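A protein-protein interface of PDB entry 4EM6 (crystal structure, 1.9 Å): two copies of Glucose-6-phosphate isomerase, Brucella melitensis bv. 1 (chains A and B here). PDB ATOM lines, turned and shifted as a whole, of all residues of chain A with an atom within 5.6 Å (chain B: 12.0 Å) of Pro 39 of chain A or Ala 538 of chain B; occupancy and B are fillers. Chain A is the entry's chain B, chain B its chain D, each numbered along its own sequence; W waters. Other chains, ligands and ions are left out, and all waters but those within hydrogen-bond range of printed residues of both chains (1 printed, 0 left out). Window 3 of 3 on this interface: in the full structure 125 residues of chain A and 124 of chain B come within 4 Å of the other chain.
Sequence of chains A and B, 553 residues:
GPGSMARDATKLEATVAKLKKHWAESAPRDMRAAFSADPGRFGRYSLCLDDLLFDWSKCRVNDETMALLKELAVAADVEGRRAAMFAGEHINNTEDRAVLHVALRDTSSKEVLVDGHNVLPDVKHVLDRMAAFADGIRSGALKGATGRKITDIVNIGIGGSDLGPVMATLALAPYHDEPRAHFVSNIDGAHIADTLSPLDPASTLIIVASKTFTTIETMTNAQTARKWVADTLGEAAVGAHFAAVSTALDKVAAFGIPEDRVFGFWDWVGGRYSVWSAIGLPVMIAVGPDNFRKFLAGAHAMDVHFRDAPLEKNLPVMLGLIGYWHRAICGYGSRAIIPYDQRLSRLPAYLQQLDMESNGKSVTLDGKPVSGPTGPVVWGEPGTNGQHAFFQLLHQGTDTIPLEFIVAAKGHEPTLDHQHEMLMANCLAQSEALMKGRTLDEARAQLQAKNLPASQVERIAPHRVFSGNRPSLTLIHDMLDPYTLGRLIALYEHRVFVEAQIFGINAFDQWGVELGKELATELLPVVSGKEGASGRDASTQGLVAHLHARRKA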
ATOM      1  N   ALA A  34     -37.064  19.941  -3.189  1.00  0.00           N
ATOM      2  CA  ALA A  34     -35.792  19.271  -3.420  1.00  0.00           C
ATOM      3  C   ALA A  34     -34.648  20.219  -3.111  1.00  0.00           C
ATOM      4  O   ALA A  34     -33.696  19.850  -2.398  1.00  0.00           O
ATOM      5  CB  ALA A  34     -35.695  18.780  -4.834  1.00  0.00           C
ATOM      6  N   PHE A  35     -34.740  21.450  -3.614  1.00  0.00           N
ATOM      7  CA  PHE A  35     -33.688  22.423  -3.332  1.00  0.00           C
ATOM      8  C   PHE A  35     -33.647  22.795  -1.872  1.00  0.00           C
ATOM      9  O   PHE A  35     -32.571  22.979  -1.324  1.00  0.00           O
ATOM     10  CB  PHE A  35     -33.808  23.678  -4.205  1.00  0.00           C
ATOM     11  CG  PHE A  35     -33.110  23.543  -5.524  1.00  0.00           C
ATOM     12  CD1 PHE A  35     -31.736  23.683  -5.611  1.00  0.00           C
ATOM     13  CD2 PHE A  35     -33.823  23.230  -6.676  1.00  0.00           C
ATOM     14  CE1 PHE A  35     -31.091  23.542  -6.827  1.00  0.00           C
ATOM     15  CE2 PHE A  35     -33.184  23.104  -7.902  1.00  0.00           C
ATOM     16  CZ  PHE A  35     -31.831  23.241  -7.971  1.00  0.00           C
ATOM     17  N   SER A  36     -34.815  22.920  -1.246  1.00  0.00           N
ATOM     18  CA  SER A  36     -34.869  23.277   0.163  1.00  0.00           C
ATOM     19  C   SER A  36     -34.184  22.220   1.048  1.00  0.00           C
ATOM     20  O   SER A  36     -33.376  22.558   1.921  1.00  0.00           O
ATOM     21  CB  SER A  36     -36.320  23.474   0.616  1.00  0.00           C
ATOM     22  OG  SER A  36     -36.345  23.915   1.959  1.00  0.00           O
ATOM     23  N   ALA A  37     -34.516  20.955   0.821  1.00  0.00           N
ATOM     24  CA  ALA A  37     -34.001  19.854   1.613  1.00  0.00           C
ATOM     25  C   ALA A  37     -32.576  19.469   1.259  1.00  0.00           C
ATOM     26  O   ALA A  37     -31.901  18.870   2.082  1.00  0.00           O
ATOM     27  CB  ALA A  37     -34.894  18.633   1.450  1.00  0.00           C
ATOM     28  N   ASP A  38     -32.118  19.823   0.064  1.00  0.00           N
ATOM     29  CA  ASP A  38     -30.904  19.275  -0.524  1.00  0.00           C
ATOM     30  C   ASP A  38     -30.157  20.327  -1.369  1.00  0.00           C
ATOM     31  O   ASP A  38     -30.060  20.200  -2.593  1.00  0.00           O
ATOM     32  CB  ASP A  38     -31.272  18.053  -1.374  1.00  0.00           C
ATOM     33  CG  ASP A  38     -30.070  17.351  -1.974  1.00  0.00           C
ATOM     34  OD1 ASP A  38     -28.939  17.476  -1.431  1.00  0.00           O
ATOM     35  OD2 ASP A  38     -30.263  16.670  -3.002  1.00  0.00           O
ATOM     36  N   PRO A  39     -29.600  21.344  -0.709  1.00  0.00           N
ATOM     37  CA  PRO A  39     -28.843  22.379  -1.412  1.00  0.00           C
ATOM     38  C   PRO A  39     -27.569  21.823  -2.027  1.00  0.00           C
ATOM     39  O   PRO A  39     -27.022  22.425  -2.927  1.00  0.00           O
ATOM     40  CB  PRO A  39     -28.536  23.394  -0.316  1.00  0.00           C
ATOM     41  CG  PRO A  39     -28.758  22.679   0.962  1.00  0.00           C
ATOM     42  CD  PRO A  39     -29.777  21.656   0.721  1.00  0.00           C
ATOM     43  N   GLY A  40     -27.104  20.670  -1.535  1.00  0.00           N
ATOM     44  CA  GLY A  40     -25.992  19.954  -2.167  1.00  0.00           C
ATOM     45  C   GLY A  40     -26.220  19.575  -3.623  1.00  0.00           C
ATOM     46  O   GLY A  40     -25.255  19.268  -4.341  1.00  0.00           O
ATOM     47  N   ARG A  41     -27.467  19.602  -4.083  1.00  0.00           N
ATOM     48  CA  ARG A  41     -27.749  19.198  -5.463  1.00  0.00           C
ATOM     49  C   ARG A  41     -27.060  20.064  -6.522  1.00  0.00           C
ATOM     50  O   ARG A  41     -26.730  19.549  -7.585  1.00  0.00           O
ATOM     51  CB  ARG A  41     -29.241  19.038  -5.744  1.00  0.00           C
ATOM     52  CG  ARG A  41     -30.063  20.279  -5.759  1.00  0.00           C
ATOM     53  CD  ARG A  41     -31.557  19.916  -5.994  1.00  0.00           C
ATOM     54  NE  ARG A  41     -31.827  19.530  -7.380  1.00  0.00           N
ATOM     55  CZ  ARG A  41     -32.119  18.295  -7.812  1.00  0.00           C
ATOM     56  NH1 ARG A  41     -32.249  17.259  -6.976  1.00  0.00           N
ATOM     57  NH2 ARG A  41     -32.301  18.096  -9.112  1.00  0.00           N
ATOM     58  N   PHE A  42     -26.819  21.348  -6.233  1.00  0.00           N
ATOM     59  CA  PHE A  42     -26.056  22.182  -7.168  1.00  0.00           C
ATOM     60  C   PHE A  42     -24.692  21.568  -7.411  1.00  0.00           C
ATOM     61  O   PHE A  42     -24.292  21.369  -8.556  1.00  0.00           O
ATOM     62  CB  PHE A  42     -25.857  23.621  -6.680  1.00  0.00           C
ATOM     63  CG  PHE A  42     -24.919  24.409  -7.545  1.00  0.00           C
ATOM     64  CD1 PHE A  42     -25.306  24.802  -8.820  1.00  0.00           C
ATOM     65  CD2 PHE A  42     -23.641  24.701  -7.123  1.00  0.00           C
ATOM     66  CE1 PHE A  42     -24.461  25.529  -9.626  1.00  0.00           C
ATOM     67  CE2 PHE A  42     -22.786  25.412  -7.932  1.00  0.00           C
ATOM     68  CZ  PHE A  42     -23.205  25.833  -9.193  1.00  0.00           C
ATOM     69  N   GLY A  43     -23.965  21.276  -6.337  1.00  0.00           N
ATOM     70  CA  GLY A  43     -22.639  20.698  -6.492  1.00  0.00           C
ATOM     71  C   GLY A  43     -22.666  19.343  -7.186  1.00  0.00           C
ATOM     72  O   GLY A  43     -21.799  19.042  -8.021  1.00  0.00           O
ATOM     73  N   SER A  57     -28.622  21.173 -12.272  1.00  0.00           N
ATOM     74  CA  SER A  57     -29.283  20.851 -10.997  1.00  0.00           C
ATOM     75  C   SER A  57     -30.770  21.243 -10.958  1.00  0.00           C
ATOM     76  O   SER A  57     -31.498  20.764 -10.087  1.00  0.00           O
ATOM     77  CB  SER A  57     -28.526  21.456  -9.806  1.00  0.00           C
ATOM     78  OG  SER A  57     -28.576  22.855  -9.827  1.00  0.00           O
ATOM     79  N   LEU B 523     -33.088  39.927  -8.634  1.00  0.00           N
ATOM     80  CA  LEU B 523     -31.758  39.327  -8.799  1.00  0.00           C
ATOM     81  C   LEU B 523     -30.678  40.311  -9.224  1.00  0.00           C
ATOM     82  O   LEU B 523     -29.518  40.062  -8.959  1.00  0.00           O
ATOM     83  CB  LEU B 523     -31.778  38.193  -9.816  1.00  0.00           C
ATOM     84  CG  LEU B 523     -31.900  36.782  -9.280  1.00  0.00           C
ATOM     85  CD1 LEU B 523     -32.061  35.825 -10.482  1.00  0.00           C
ATOM     86  CD2 LEU B 523     -30.667  36.417  -8.389  1.00  0.00           C
ATOM     87  N   VAL B 526     -28.213  41.410  -6.607  1.00  0.00           N
ATOM     88  CA  VAL B 526     -27.477  40.262  -6.104  1.00  0.00           C
ATOM     89  C   VAL B 526     -26.395  39.907  -7.124  1.00  0.00           C
ATOM     90  O   VAL B 526     -25.244  39.645  -6.762  1.00  0.00           O
ATOM     91  CB  VAL B 526     -28.421  39.063  -5.825  1.00  0.00           C
ATOM     92  CG1 VAL B 526     -27.617  37.745  -5.523  1.00  0.00           C
ATOM     93  CG2 VAL B 526     -29.388  39.402  -4.645  1.00  0.00           C
ATOM     94  N   ALA B 533     -26.298  37.898  -0.233  1.00  0.00           N
ATOM     95  CA  ALA B 533     -27.210  36.810  -0.577  1.00  0.00           C
ATOM     96  C   ALA B 533     -28.462  36.924   0.285  1.00  0.00           C
ATOM     97  O   ALA B 533     -28.425  37.534   1.361  1.00  0.00           O
ATOM     98  CB  ALA B 533     -26.532  35.456  -0.350  1.00  0.00           C
ATOM     99  N   SER B 534     -29.567  36.357  -0.203  1.00  0.00           N
ATOM    100  CA  SER B 534     -30.784  36.281   0.595  1.00  0.00           C
ATOM    101  C   SER B 534     -31.648  35.067   0.242  1.00  0.00           C
ATOM    102  O   SER B 534     -32.796  35.210  -0.177  1.00  0.00           O
ATOM    103  CB  SER B 534     -31.582  37.611   0.552  1.00  0.00           C
ATOM    104  OG  SER B 534     -31.755  38.107  -0.765  1.00  0.00           O
ATOM    105  N   GLY B 535     -31.056  33.886   0.381  1.00  0.00           N
ATOM    106  CA  GLY B 535     -31.808  32.641   0.527  1.00  0.00           C
ATOM    107  C   GLY B 535     -32.516  32.066  -0.690  1.00  0.00           C
ATOM    108  O   GLY B 535     -33.526  31.385  -0.557  1.00  0.00           O
ATOM    109  N   ARG B 536     -31.979  32.297  -1.878  1.00  0.00           N
ATOM    110  CA  ARG B 536     -32.522  31.670  -3.087  1.00  0.00           C
ATOM    111  C   ARG B 536     -32.058  30.224  -3.159  1.00  0.00           C
ATOM    112  O   ARG B 536     -31.233  29.784  -2.350  1.00  0.00           O
ATOM    113  CB  ARG B 536     -32.086  32.452  -4.324  1.00  0.00           C
ATOM    114  CG  ARG B 536     -32.707  33.836  -4.329  1.00  0.00           C
ATOM    115  CD  ARG B 536     -32.431  34.647  -5.562  1.00  0.00           C
ATOM    116  NE  ARG B 536     -33.260  35.840  -5.504  1.00  0.00           N
ATOM    117  CZ  ARG B 536     -33.060  36.869  -4.674  1.00  0.00           C
ATOM    118  NH1 ARG B 536     -32.025  36.920  -3.822  1.00  0.00           N
ATOM    119  NH2 ARG B 536     -33.919  37.868  -4.682  1.00  0.00           N
ATOM    120  N   ASP B 537     -32.568  29.493  -4.135  1.00  0.00           N
ATOM    121  CA  ASP B 537     -32.207  28.074  -4.311  1.00  0.00           C
ATOM    122  C   ASP B 537     -30.709  27.912  -4.598  1.00  0.00           C
ATOM    123  O   ASP B 537     -30.050  28.833  -5.082  1.00  0.00           O
ATOM    124  CB  ASP B 537     -33.050  27.451  -5.432  1.00  0.00           C
ATOM    125  CG  ASP B 537     -32.656  27.953  -6.804  1.00  0.00           C
ATOM    126  OD1 ASP B 537     -31.691  27.391  -7.348  1.00  0.00           O
ATOM    127  OD2 ASP B 537     -33.291  28.896  -7.345  1.00  0.00           O
ATOM    128  N   ALA B 538     -30.177  26.733  -4.307  1.00  0.00           N
ATOM    129  CA  ALA B 538     -28.751  26.499  -4.400  1.00  0.00           C
ATOM    130  C   ALA B 538     -28.200  26.629  -5.813  1.00  0.00           C
ATOM    131  O   ALA B 538     -27.010  26.902  -5.966  1.00  0.00           O
ATOM    132  CB  ALA B 538     -28.375  25.143  -3.807  1.00  0.00           C
ATOM    133  N   SER B 539     -29.033  26.422  -6.828  1.00  0.00           N
ATOM    134  CA  SER B 539     -28.568  26.574  -8.197  1.00  0.00           C
ATOM    135  C   SER B 539     -28.404  28.066  -8.511  1.00  0.00           C
ATOM    136  O   SER B 539     -27.345  28.488  -8.958  1.00  0.00           O
ATOM    137  CB  SER B 539     -29.519  25.918  -9.198  1.00  0.00           C
ATOM    138  OG  SER B 539     -29.128  26.209 -10.549  1.00  0.00           O
ATOM    139  N   THR B 540     -29.441  28.856  -8.235  1.00  0.00           N
ATOM    140  CA  THR B 540     -29.350  30.300  -8.428  1.00  0.00           C
ATOM    141  C   THR B 540     -28.148  30.835  -7.648  1.00  0.00           C
ATOM    142  O   THR B 540     -27.342  31.574  -8.189  1.00  0.00           O
ATOM    143  CB  THR B 540     -30.650  31.010  -8.023  1.00  0.00           C
ATOM    144  OG1 THR B 540     -31.727  30.519  -8.832  1.00  0.00           O
ATOM    145  CG2 THR B 540     -30.526  32.502  -8.211  1.00  0.00           C
ATOM    146  N   GLN B 541     -27.997  30.419  -6.408  1.00  0.00           N
ATOM    147  CA  GLN B 541     -26.894  30.861  -5.600  1.00  0.00           C
ATOM    148  C   GLN B 541     -25.569  30.462  -6.233  1.00  0.00           C
ATOM    149  O   GLN B 541     -24.714  31.229  -6.348  1.00  0.00           O
ATOM    150  CB  GLN B 541     -27.064  30.360  -4.158  1.00  0.00           C
ATOM    151  CG  GLN B 541     -28.224  30.986  -3.486  1.00  0.00           C
ATOM    152  CD  GLN B 541     -28.044  31.133  -1.969  1.00  0.00           C
ATOM    153  OE1 GLN B 541     -28.411  32.075  -1.457  1.00  0.00           O
ATOM    154  NE2 GLN B 541     -27.472  30.158  -1.317  1.00  0.00           N
ATOM    155  N   GLY B 542     -25.483  29.216  -6.659  1.00  0.00           N
ATOM    156  CA  GLY B 542     -24.261  28.675  -7.269  1.00  0.00           C
ATOM    157  C   GLY B 542     -23.831  29.406  -8.528  1.00  0.00           C
ATOM    158  O   GLY B 542     -22.635  29.671  -8.723  1.00  0.00           O
ATOM    159  N   LEU B 543     -24.816  29.722  -9.375  1.00  0.00           N
ATOM    160  CA  LEU B 543     -24.583  30.481 -10.597  1.00  0.00           C
ATOM    161  C   LEU B 543     -24.137  31.924 -10.290  1.00  0.00           C
ATOM    162  O   LEU B 543     -23.156  32.409 -10.861  1.00  0.00           O
ATOM    163  CB  LEU B 543     -25.821  30.449 -11.483  1.00  0.00           C
ATOM    164  CG  LEU B 543     -26.260  29.063 -11.978  1.00  0.00           C
ATOM    165  CD1 LEU B 543     -27.608  29.168 -12.648  1.00  0.00           C
ATOM    166  CD2 LEU B 543     -25.216  28.429 -12.912  1.00  0.00           C
ATOM    167  N   VAL B 544     -24.805  32.572  -9.335  1.00  0.00           N
ATOM    168  CA  VAL B 544     -24.379  33.889  -8.843  1.00  0.00           C
ATOM    169  C   VAL B 544     -22.940  33.872  -8.322  1.00  0.00           C
ATOM    170  O   VAL B 544     -22.146  34.755  -8.669  1.00  0.00           O
ATOM    171  CB  VAL B 544     -25.317  34.422  -7.726  1.00  0.00           C
ATOM    172  CG1 VAL B 544     -24.686  35.609  -7.032  1.00  0.00           C
ATOM    173  CG2 VAL B 544     -26.729  34.815  -8.290  1.00  0.00           C
ATOM    174  N   ALA B 545     -22.604  32.880  -7.489  1.00  0.00           N
ATOM    175  CA  ALA B 545     -21.252  32.775  -6.920  1.00  0.00           C
ATOM    176  C   ALA B 545     -20.202  32.584  -8.022  1.00  0.00           C
ATOM    177  O   ALA B 545     -19.117  33.168  -7.966  1.00  0.00           O
ATOM    178  CB  ALA B 545     -21.167  31.637  -5.875  1.00  0.00           C
ATOM    179  N   HIS B 546     -20.542  31.766  -9.013  1.00  0.00           N
ATOM    180  CA  HIS B 546     -19.659  31.561 -10.159  1.00  0.00           C
ATOM    181  C   HIS B 546     -19.440  32.894 -10.881  1.00  0.00           C
ATOM    182  O   HIS B 546     -18.299  33.298 -11.137  1.00  0.00           O
ATOM    183  CB  HIS B 546     -20.232  30.505 -11.112  1.00  0.00           C
ATOM    184  CG  HIS B 546     -19.427  30.339 -12.365  1.00  0.00           C
ATOM    185  ND1 HIS B 546     -18.287  29.560 -12.419  1.00  0.00           N
ATOM    186  CD2 HIS B 546     -19.570  30.885 -13.594  1.00  0.00           C
ATOM    187  CE1 HIS B 546     -17.762  29.639 -13.633  1.00  0.00           C
ATOM    188  NE2 HIS B 546     -18.525  30.430 -14.367  1.00  0.00           N
ATOM    189  N   LEU B 547     -20.524  33.608 -11.178  1.00  0.00           N
ATOM    190  CA  LEU B 547     -20.381  34.882 -11.871  1.00  0.00           C
ATOM    191  C   LEU B 547     -19.476  35.841 -11.104  1.00  0.00           C
ATOM    192  O   LEU B 547     -18.557  36.451 -11.685  1.00  0.00           O
ATOM    193  CB  LEU B 547     -21.749  35.512 -12.140  1.00  0.00           C
ATOM    194  CG  LEU B 547     -22.618  34.769 -13.158  1.00  0.00           C
ATOM    195  CD1 LEU B 547     -24.045  35.335 -13.138  1.00  0.00           C
ATOM    196  CD2 LEU B 547     -22.047  34.806 -14.573  1.00  0.00           C
HETATM  197  O   HOH W   1     -31.384  25.424  -2.067  1.00  0.00           O
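OG of Ser 57 of chain A lies close to OG of Ser 539 of chain B (3.5 Å).
OD1 of Asp 537 of chain B sits at hydrogen-bond distance from N of Ser 539 of chain B. The side-chain hydroxyl (OG1) of Thr 540 of chain B is in hydrogen-bond range of the side-chain carboxylate (OD2) of Asp 537 of chain B, at 2.7 Å. O of Ser 57 of chain A is in hydrogen-bond range of NH2 of Arg 41 of chain A (3.0 Å).
Phe 35 of chain A touches Asp 537 of chain B (CG to CB, 3.9 Å). Ala 538 of chain B touches Phe 35 of chain A. Ser 539 of chain B touches Phe 35 of chain A (N to CE1, 3.5 Å). O of Pro 39 of chain A touches CB of Ala 538 of chain B, 3.2 Å away. O of Ala 538 of chain B touches CB of Phe 42 of chain A, 3.6 Å away. Phe 42 of chain A touches Ser 539 of chain B (CD1 to CA, 3.8 Å). CA of Gly 542 of chain B touches CZ of Phe 42 of chain A, 3.6 Å away.
Of chain B, only Ala 538 comes within 4 Å of Pro 39 of chain A. Ala 538 of chain B touches three residues of chain A. Ser 36 of chain A touches none of the printed residues of chain B. No residue of chain B comes within 4 Å of Ala 37 of chain A. No residue of chain B comes within 4 Å of Asp 38 of chain A. No residue of chain B comes within 4 Å of Gly 40 of chain A. Of chain B, only Ala 538, Ser 539 and Gly 542 come within 4 Å of Phe 42 of chain A. Printed residues of chain A within 4 Å of Ser 539 of chain B: Phe 35 (3.5 Å), Phe 42 (3.8 Å) and Ser 57 (3.3 Å). Of the printed residues of chain B, Ser 57 of chain A touches Ser 539. Of the printed residues of chain A, Gly 542 of chain B touches Phe 42. Leu 543 of chain B touches none of the printed residues of chain A. The nearest residue of chain B that does not touch Pro 39 of chain A is Ser 539 of chain B (5.9 Å). The nearest residue of chain A that does not touch Ala 538 of chain B is Gly 40 of chain A (5.2 Å).
Of the 11 printed residues of chain A, 4 touch a printed residue of chain B. Hydrophobic or aromatic side chains of chain A within 4 Å of the printed part of chain B: Phe 35, Pro 39 and Phe 42. Of the 17 printed residues of chain B, 4 touch a printed residue of chain A. Hydrophobic or aromatic side chains of chain B that line the printed part of chain A: Ala 538. Among the printed residues, 8 pairs touch across the chains. Among the printed residues, no Asp or Glu carboxylate lies within 4 Å of a Lys or Arg side-chain nitrogen of the other chain.
No position is printed for both chains. Of the 8 pairs that touch across the chains among the printed residues, none has its exchanged pair printed and touching as well.
Water W1 lies within hydrogen-bond range of the backbone carbonyl oxygen (O) of Phe 35 of chain A (2.8 Å) and the backbone NH (N) of Ala 538 of chain B (2.9 Å).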
